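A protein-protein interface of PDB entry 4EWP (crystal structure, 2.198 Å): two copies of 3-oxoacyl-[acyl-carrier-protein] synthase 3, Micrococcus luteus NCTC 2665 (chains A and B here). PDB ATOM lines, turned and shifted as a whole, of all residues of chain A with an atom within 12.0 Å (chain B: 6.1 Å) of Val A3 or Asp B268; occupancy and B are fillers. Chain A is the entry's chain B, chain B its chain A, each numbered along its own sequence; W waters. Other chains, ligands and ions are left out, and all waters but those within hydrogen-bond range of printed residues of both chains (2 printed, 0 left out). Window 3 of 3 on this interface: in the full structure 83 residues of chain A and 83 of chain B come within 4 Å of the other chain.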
ATOM      1  N   THR A   2     -15.031  35.512 -25.322  1.00  0.00           N
ATOM      2  CA  THR A   2     -14.559  35.003 -26.606  1.00  0.00           C
ATOM      3  C   THR A   2     -15.738  34.789 -27.561  1.00  0.00           C
ATOM      4  O   THR A   2     -15.980  35.609 -28.450  1.00  0.00           O
ATOM      5  CB  THR A   2     -13.755  33.693 -26.435  1.00  0.00           C
ATOM      6  OG1 THR A   2     -13.015  33.738 -25.207  1.00  0.00           O
ATOM      7  CG2 THR A   2     -12.787  33.495 -27.598  1.00  0.00           C
ATOM      8  N   VAL A   3     -16.475  33.696 -27.370  1.00  0.00           N
ATOM      9  CA  VAL A   3     -17.654  33.424 -28.194  1.00  0.00           C
ATOM     10  C   VAL A   3     -18.956  33.740 -27.458  1.00  0.00           C
ATOM     11  O   VAL A   3     -19.267  33.134 -26.430  1.00  0.00           O
ATOM     12  CB  VAL A   3     -17.685  31.961 -28.695  1.00  0.00           C
ATOM     13  CG1 VAL A   3     -18.973  31.686 -29.455  1.00  0.00           C
ATOM     14  CG2 VAL A   3     -16.476  31.672 -29.576  1.00  0.00           C
ATOM     15  N   THR A   4     -19.716  34.691 -27.993  1.00  0.00           N
ATOM     16  CA  THR A   4     -21.000  35.064 -27.414  1.00  0.00           C
ATOM     17  C   THR A   4     -22.163  34.363 -28.121  1.00  0.00           C
ATOM     18  O   THR A   4     -22.324  34.484 -29.337  1.00  0.00           O
ATOM     19  CB  THR A   4     -21.232  36.581 -27.473  1.00  0.00           C
ATOM     20  OG1 THR A   4     -20.098  37.270 -26.928  1.00  0.00           O
ATOM     21  CG2 THR A   4     -22.483  36.951 -26.688  1.00  0.00           C
ATOM     22  N   LEU A   5     -22.967  33.638 -27.351  1.00  0.00           N
ATOM     23  CA  LEU A   5     -24.086  32.889 -27.895  1.00  0.00           C
ATOM     24  C   LEU A   5     -25.178  33.820 -28.377  1.00  0.00           C
ATOM     25  O   LEU A   5     -25.446  34.845 -27.756  1.00  0.00           O
ATOM     26  CB  LEU A   5     -24.677  31.958 -26.843  1.00  0.00           C
ATOM     27  CG  LEU A   5     -23.798  30.866 -26.248  1.00  0.00           C
ATOM     28  CD1 LEU A   5     -24.597  30.123 -25.173  1.00  0.00           C
ATOM     29  CD2 LEU A   5     -23.323  29.911 -27.335  1.00  0.00           C
ATOM     30  N   LYS A   6     -25.817  33.447 -29.481  1.00  0.00           N
ATOM     31  CA  LYS A   6     -26.907  34.235 -30.035  1.00  0.00           C
ATOM     32  C   LYS A   6     -28.136  34.014 -29.183  1.00  0.00           C
ATOM     33  O   LYS A   6     -28.241  33.006 -28.485  1.00  0.00           O
ATOM     34  CB  LYS A   6     -27.183  33.843 -31.492  1.00  0.00           C
ATOM     35  CG  LYS A   6     -26.042  34.164 -32.462  1.00  0.00           C
ATOM     36  CD  LYS A   6     -26.482  33.944 -33.898  1.00  0.00           C
ATOM     37  CE  LYS A   6     -25.519  34.584 -34.890  1.00  0.00           C
ATOM     38  NZ  LYS A   6     -24.140  34.015 -34.843  1.00  0.00           N
ATOM     39  N   GLN A   7     -29.062  34.964 -29.227  1.00  0.00           N
ATOM     40  CA  GLN A   7     -30.284  34.862 -28.438  1.00  0.00           C
ATOM     41  C   GLN A   7     -31.473  35.275 -29.288  1.00  0.00           C
ATOM     42  O   GLN A   7     -31.339  36.107 -30.189  1.00  0.00           O
ATOM     43  CB  GLN A   7     -30.186  35.725 -27.171  1.00  0.00           C
ATOM     44  CG  GLN A   7     -29.091  35.278 -26.194  1.00  0.00           C
ATOM     45  CD  GLN A   7     -29.499  34.068 -25.374  1.00  0.00           C
ATOM     46  OE1 GLN A   7     -30.087  34.218 -24.305  1.00  0.00           O
ATOM     47  NE2 GLN A   7     -29.197  32.857 -25.875  1.00  0.00           N
ATOM     48  N   ALA B 262     -26.988  29.030 -32.536  1.00  0.00           N
ATOM     49  CA  ALA B 262     -26.178  29.499 -31.416  1.00  0.00           C
ATOM     50  C   ALA B 262     -25.136  30.514 -31.883  1.00  0.00           C
ATOM     51  O   ALA B 262     -24.661  31.346 -31.100  1.00  0.00           O
ATOM     52  CB  ALA B 262     -25.510  28.318 -30.699  1.00  0.00           C
ATOM     53  N   GLY B 263     -24.787  30.443 -33.165  1.00  0.00           N
ATOM     54  CA  GLY B 263     -23.724  31.261 -33.716  1.00  0.00           C
ATOM     55  C   GLY B 263     -22.345  30.705 -33.391  1.00  0.00           C
ATOM     56  O   GLY B 263     -21.421  31.448 -33.050  1.00  0.00           O
ATOM     57  N   VAL B 264     -22.206  29.390 -33.522  1.00  0.00           N
ATOM     58  CA  VAL B 264     -21.062  28.672 -32.977  1.00  0.00           C
ATOM     59  C   VAL B 264     -20.594  27.601 -33.966  1.00  0.00           C
ATOM     60  O   VAL B 264     -21.405  27.025 -34.692  1.00  0.00           O
ATOM     61  CB  VAL B 264     -21.450  28.062 -31.589  1.00  0.00           C
ATOM     62  CG1 VAL B 264     -20.672  26.808 -31.276  1.00  0.00           C
ATOM     63  CG2 VAL B 264     -21.299  29.106 -30.481  1.00  0.00           C
ATOM     64  N   GLU B 265     -19.287  27.363 -34.024  1.00  0.00           N
ATOM     65  CA  GLU B 265     -18.735  26.307 -34.872  1.00  0.00           C
ATOM     66  C   GLU B 265     -18.243  25.178 -33.973  1.00  0.00           C
ATOM     67  O   GLU B 265     -17.966  25.411 -32.797  1.00  0.00           O
ATOM     68  CB  GLU B 265     -17.575  26.844 -35.711  1.00  0.00           C
ATOM     69  CG  GLU B 265     -17.881  28.129 -36.472  1.00  0.00           C
ATOM     70  CD  GLU B 265     -18.534  27.887 -37.824  1.00  0.00           C
ATOM     71  OE1 GLU B 265     -19.406  26.999 -37.930  1.00  0.00           O
ATOM     72  OE2 GLU B 265     -18.163  28.589 -38.791  1.00  0.00           O
ATOM     73  N   PRO B 266     -18.129  23.952 -34.514  1.00  0.00           N
ATOM     74  CA  PRO B 266     -17.663  22.803 -33.722  1.00  0.00           C
ATOM     75  C   PRO B 266     -16.320  23.065 -33.014  1.00  0.00           C
ATOM     76  O   PRO B 266     -16.070  22.528 -31.929  1.00  0.00           O
ATOM     77  CB  PRO B 266     -17.504  21.703 -34.774  1.00  0.00           C
ATOM     78  CG  PRO B 266     -18.461  22.083 -35.848  1.00  0.00           C
ATOM     79  CD  PRO B 266     -18.398  23.580 -35.913  1.00  0.00           C
ATOM     80  N   GLU B 267     -15.485  23.902 -33.630  1.00  0.00           N
ATOM     81  CA  GLU B 267     -14.204  24.336 -33.082  1.00  0.00           C
ATOM     82  C   GLU B 267     -14.353  25.143 -31.791  1.00  0.00           C
ATOM     83  O   GLU B 267     -13.427  25.208 -30.988  1.00  0.00           O
ATOM     84  CB  GLU B 267     -13.462  25.188 -34.123  1.00  0.00           C
ATOM     85  CG  GLU B 267     -12.925  24.410 -35.320  1.00  0.00           C
ATOM     86  CD  GLU B 267     -14.011  23.766 -36.208  1.00  0.00           C
ATOM     87  OE1 GLU B 267     -15.221  23.934 -35.958  1.00  0.00           O
ATOM     88  OE2 GLU B 267     -13.650  23.074 -37.183  1.00  0.00           O
ATOM     89  N   ASP B 268     -15.510  25.776 -31.614  1.00  0.00           N
ATOM     90  CA  ASP B 268     -15.807  26.570 -30.418  1.00  0.00           C
ATOM     91  C   ASP B 268     -16.293  25.719 -29.240  1.00  0.00           C
ATOM     92  O   ASP B 268     -16.372  26.202 -28.105  1.00  0.00           O
ATOM     93  CB  ASP B 268     -16.857  27.634 -30.744  1.00  0.00           C
ATOM     94  CG  ASP B 268     -16.380  28.624 -31.788  1.00  0.00           C
ATOM     95  OD1 ASP B 268     -15.200  29.038 -31.698  1.00  0.00           O
ATOM     96  OD2 ASP B 268     -17.174  28.979 -32.696  1.00  0.00           O
ATOM     97  N   LEU B 269     -16.627  24.459 -29.508  1.00  0.00           N
ATOM     98  CA  LEU B 269     -17.126  23.554 -28.463  1.00  0.00           C
ATOM     99  C   LEU B 269     -16.005  23.030 -27.568  1.00  0.00           C
ATOM    100  O   LEU B 269     -14.928  22.696 -28.050  1.00  0.00           O
ATOM    101  CB  LEU B 269     -17.879  22.365 -29.078  1.00  0.00           C
ATOM    102  CG  LEU B 269     -19.178  22.663 -29.837  1.00  0.00           C
ATOM    103  CD1 LEU B 269     -19.775  21.402 -30.472  1.00  0.00           C
ATOM    104  CD2 LEU B 269     -20.190  23.319 -28.897  1.00  0.00           C
ATOM    105  N   ALA B 270     -16.259  22.958 -26.264  1.00  0.00           N
ATOM    106  CA  ALA B 270     -15.365  22.247 -25.361  1.00  0.00           C
ATOM    107  C   ALA B 270     -15.839  20.810 -25.200  1.00  0.00           C
ATOM    108  O   ALA B 270     -15.066  19.929 -24.836  1.00  0.00           O
ATOM    109  CB  ALA B 270     -15.309  22.924 -24.015  1.00  0.00           C
ATOM    110  N   GLY B 329     -16.769  26.467 -20.522  1.00  0.00           N
ATOM    111  CA  GLY B 329     -16.671  26.107 -21.928  1.00  0.00           C
ATOM    112  C   GLY B 329     -18.040  25.831 -22.529  1.00  0.00           C
ATOM    113  O   GLY B 329     -19.009  25.656 -21.805  1.00  0.00           O
ATOM    114  N   LEU B 330     -18.121  25.791 -23.855  1.00  0.00           N
ATOM    115  CA  LEU B 330     -19.388  25.528 -24.537  1.00  0.00           C
ATOM    116  C   LEU B 330     -19.611  24.037 -24.782  1.00  0.00           C
ATOM    117  O   LEU B 330     -18.711  23.333 -25.240  1.00  0.00           O
ATOM    118  CB  LEU B 330     -19.448  26.267 -25.873  1.00  0.00           C
ATOM    119  CG  LEU B 330     -19.363  27.789 -25.797  1.00  0.00           C
ATOM    120  CD1 LEU B 330     -19.340  28.370 -27.202  1.00  0.00           C
ATOM    121  CD2 LEU B 330     -20.528  28.340 -24.993  1.00  0.00           C
ATOM    122  N   ARG B 348     -23.203  27.057 -21.922  1.00  0.00           N
ATOM    123  CA  ARG B 348     -21.969  27.347 -21.208  1.00  0.00           C
ATOM    124  C   ARG B 348     -21.931  26.487 -19.945  1.00  0.00           C
ATOM    125  O   ARG B 348     -22.780  26.629 -19.068  1.00  0.00           O
ATOM    126  CB  ARG B 348     -21.944  28.824 -20.843  1.00  0.00           C
ATOM    127  CG  ARG B 348     -20.623  29.310 -20.290  1.00  0.00           C
ATOM    128  CD  ARG B 348     -20.289  30.677 -20.845  1.00  0.00           C
ATOM    129  NE  ARG B 348     -19.266  30.568 -21.878  1.00  0.00           N
ATOM    130  CZ  ARG B 348     -19.330  31.156 -23.070  1.00  0.00           C
ATOM    131  NH1 ARG B 348     -20.380  31.908 -23.387  1.00  0.00           N
ATOM    132  NH2 ARG B 348     -18.343  30.988 -23.943  1.00  0.00           N
HETATM  133  O   HOH W   1     -22.193  33.819 -24.309  1.00  0.00           O
HETATM  134  O   HOH W   2     -21.757  34.427 -32.436  1.00  0.00           O
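O of Ala B262 is in hydrogen-bond range of N of Lys A6. The guanidinium group (NH2) of Arg B348 is in hydrogen-bond range of the backbone carbonyl oxygen (O) of Val A3 (3.4 Å).
Hydrophobic or aromatic side chains of chain A within 4 Å of the printed part of chain B: Val A3 and Leu A5. Among the printed residues, 8 pairs touch across the chains. Among the printed residues, no Asp or Glu carboxylate lies within 4 Å of a Lys or Arg side-chain nitrogen of the other chain.
No position is printed for both chains. Of the 8 pairs that touch across the chains among the printed residues, none has its exchanged pair printed and touching as well.
Water W1 bridges the guanidinium group of Arg B348 (2.8 Å) and the backbone NH of Leu A5 (3.1 Å). Water W2 lies within hydrogen-bond range of the backbone carbonyl oxygen of Gly B263, the backbone carbonyl oxygen of Thr A4 and the side-chain amino group of Lys A6.
Among the printed residues, pairs that only touch across the chains: Val A3 with Val B264 (3.6 Å), Val A3 with Asp B268 (3.6 Å), Leu A5 with Ala B262 (3.6 Å), Leu A5 with Val B264 (3.8 Å), Leu A5 with Leu B330 (3.97 Å) and Lys A6 with Gly B263 (3.0 Å).
Of chain B, only Val B264 (3.6 Å), Asp B268 (3.6 Å) and Arg B348 (3.4 Å) come within 4 Å of Val A3. Printed residues of chain B within 4 Å of Leu A5: Ala B262, Val B264 and Leu B330. Of the printed residues of chain B, Lys A6 touches Ala B262 (2.9 Å) and Gly B263 (3.0 Å). Of the printed residues of chain A, Ala B262 touches Leu A5 (3.6 Å) and Lys A6 (2.9 Å). Of chain A, only Lys A6 (3.0 Å) comes within 4 Å of Gly B263. Of chain A, only Val A3 (3.6 Å) and Leu A5 (3.8 Å) come within 4 Å of Val B264. Of chain A, only Val A3 comes within 4 Å of Asp B268. No residue of chain A comes within 4 Å of Leu B269. No residue of chain A comes within 4 Å of Gly B329. Leu B330 touches just one residue of chain A: Leu A5 (3.97 Å). Printed residues of chain A within 4 Å of Arg B348: Val A3 (3.4 Å). The nearest residue of chain B that does not touch Val A3 is Leu B330 (4.03 Å). The nearest residue of chain A that does not touch Asp B268 is Thr A2 (6.5 Å).
The backbone carbonyl oxygen (O) of Leu B330 sits at hydrogen-bond distance from the backbone NH (N) of Ala B270. The side-chain carboxylate (OD2) of Asp B268 sits at hydrogen-bond distance from the backbone NH (N) of Glu B265, at 3.0 Å.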
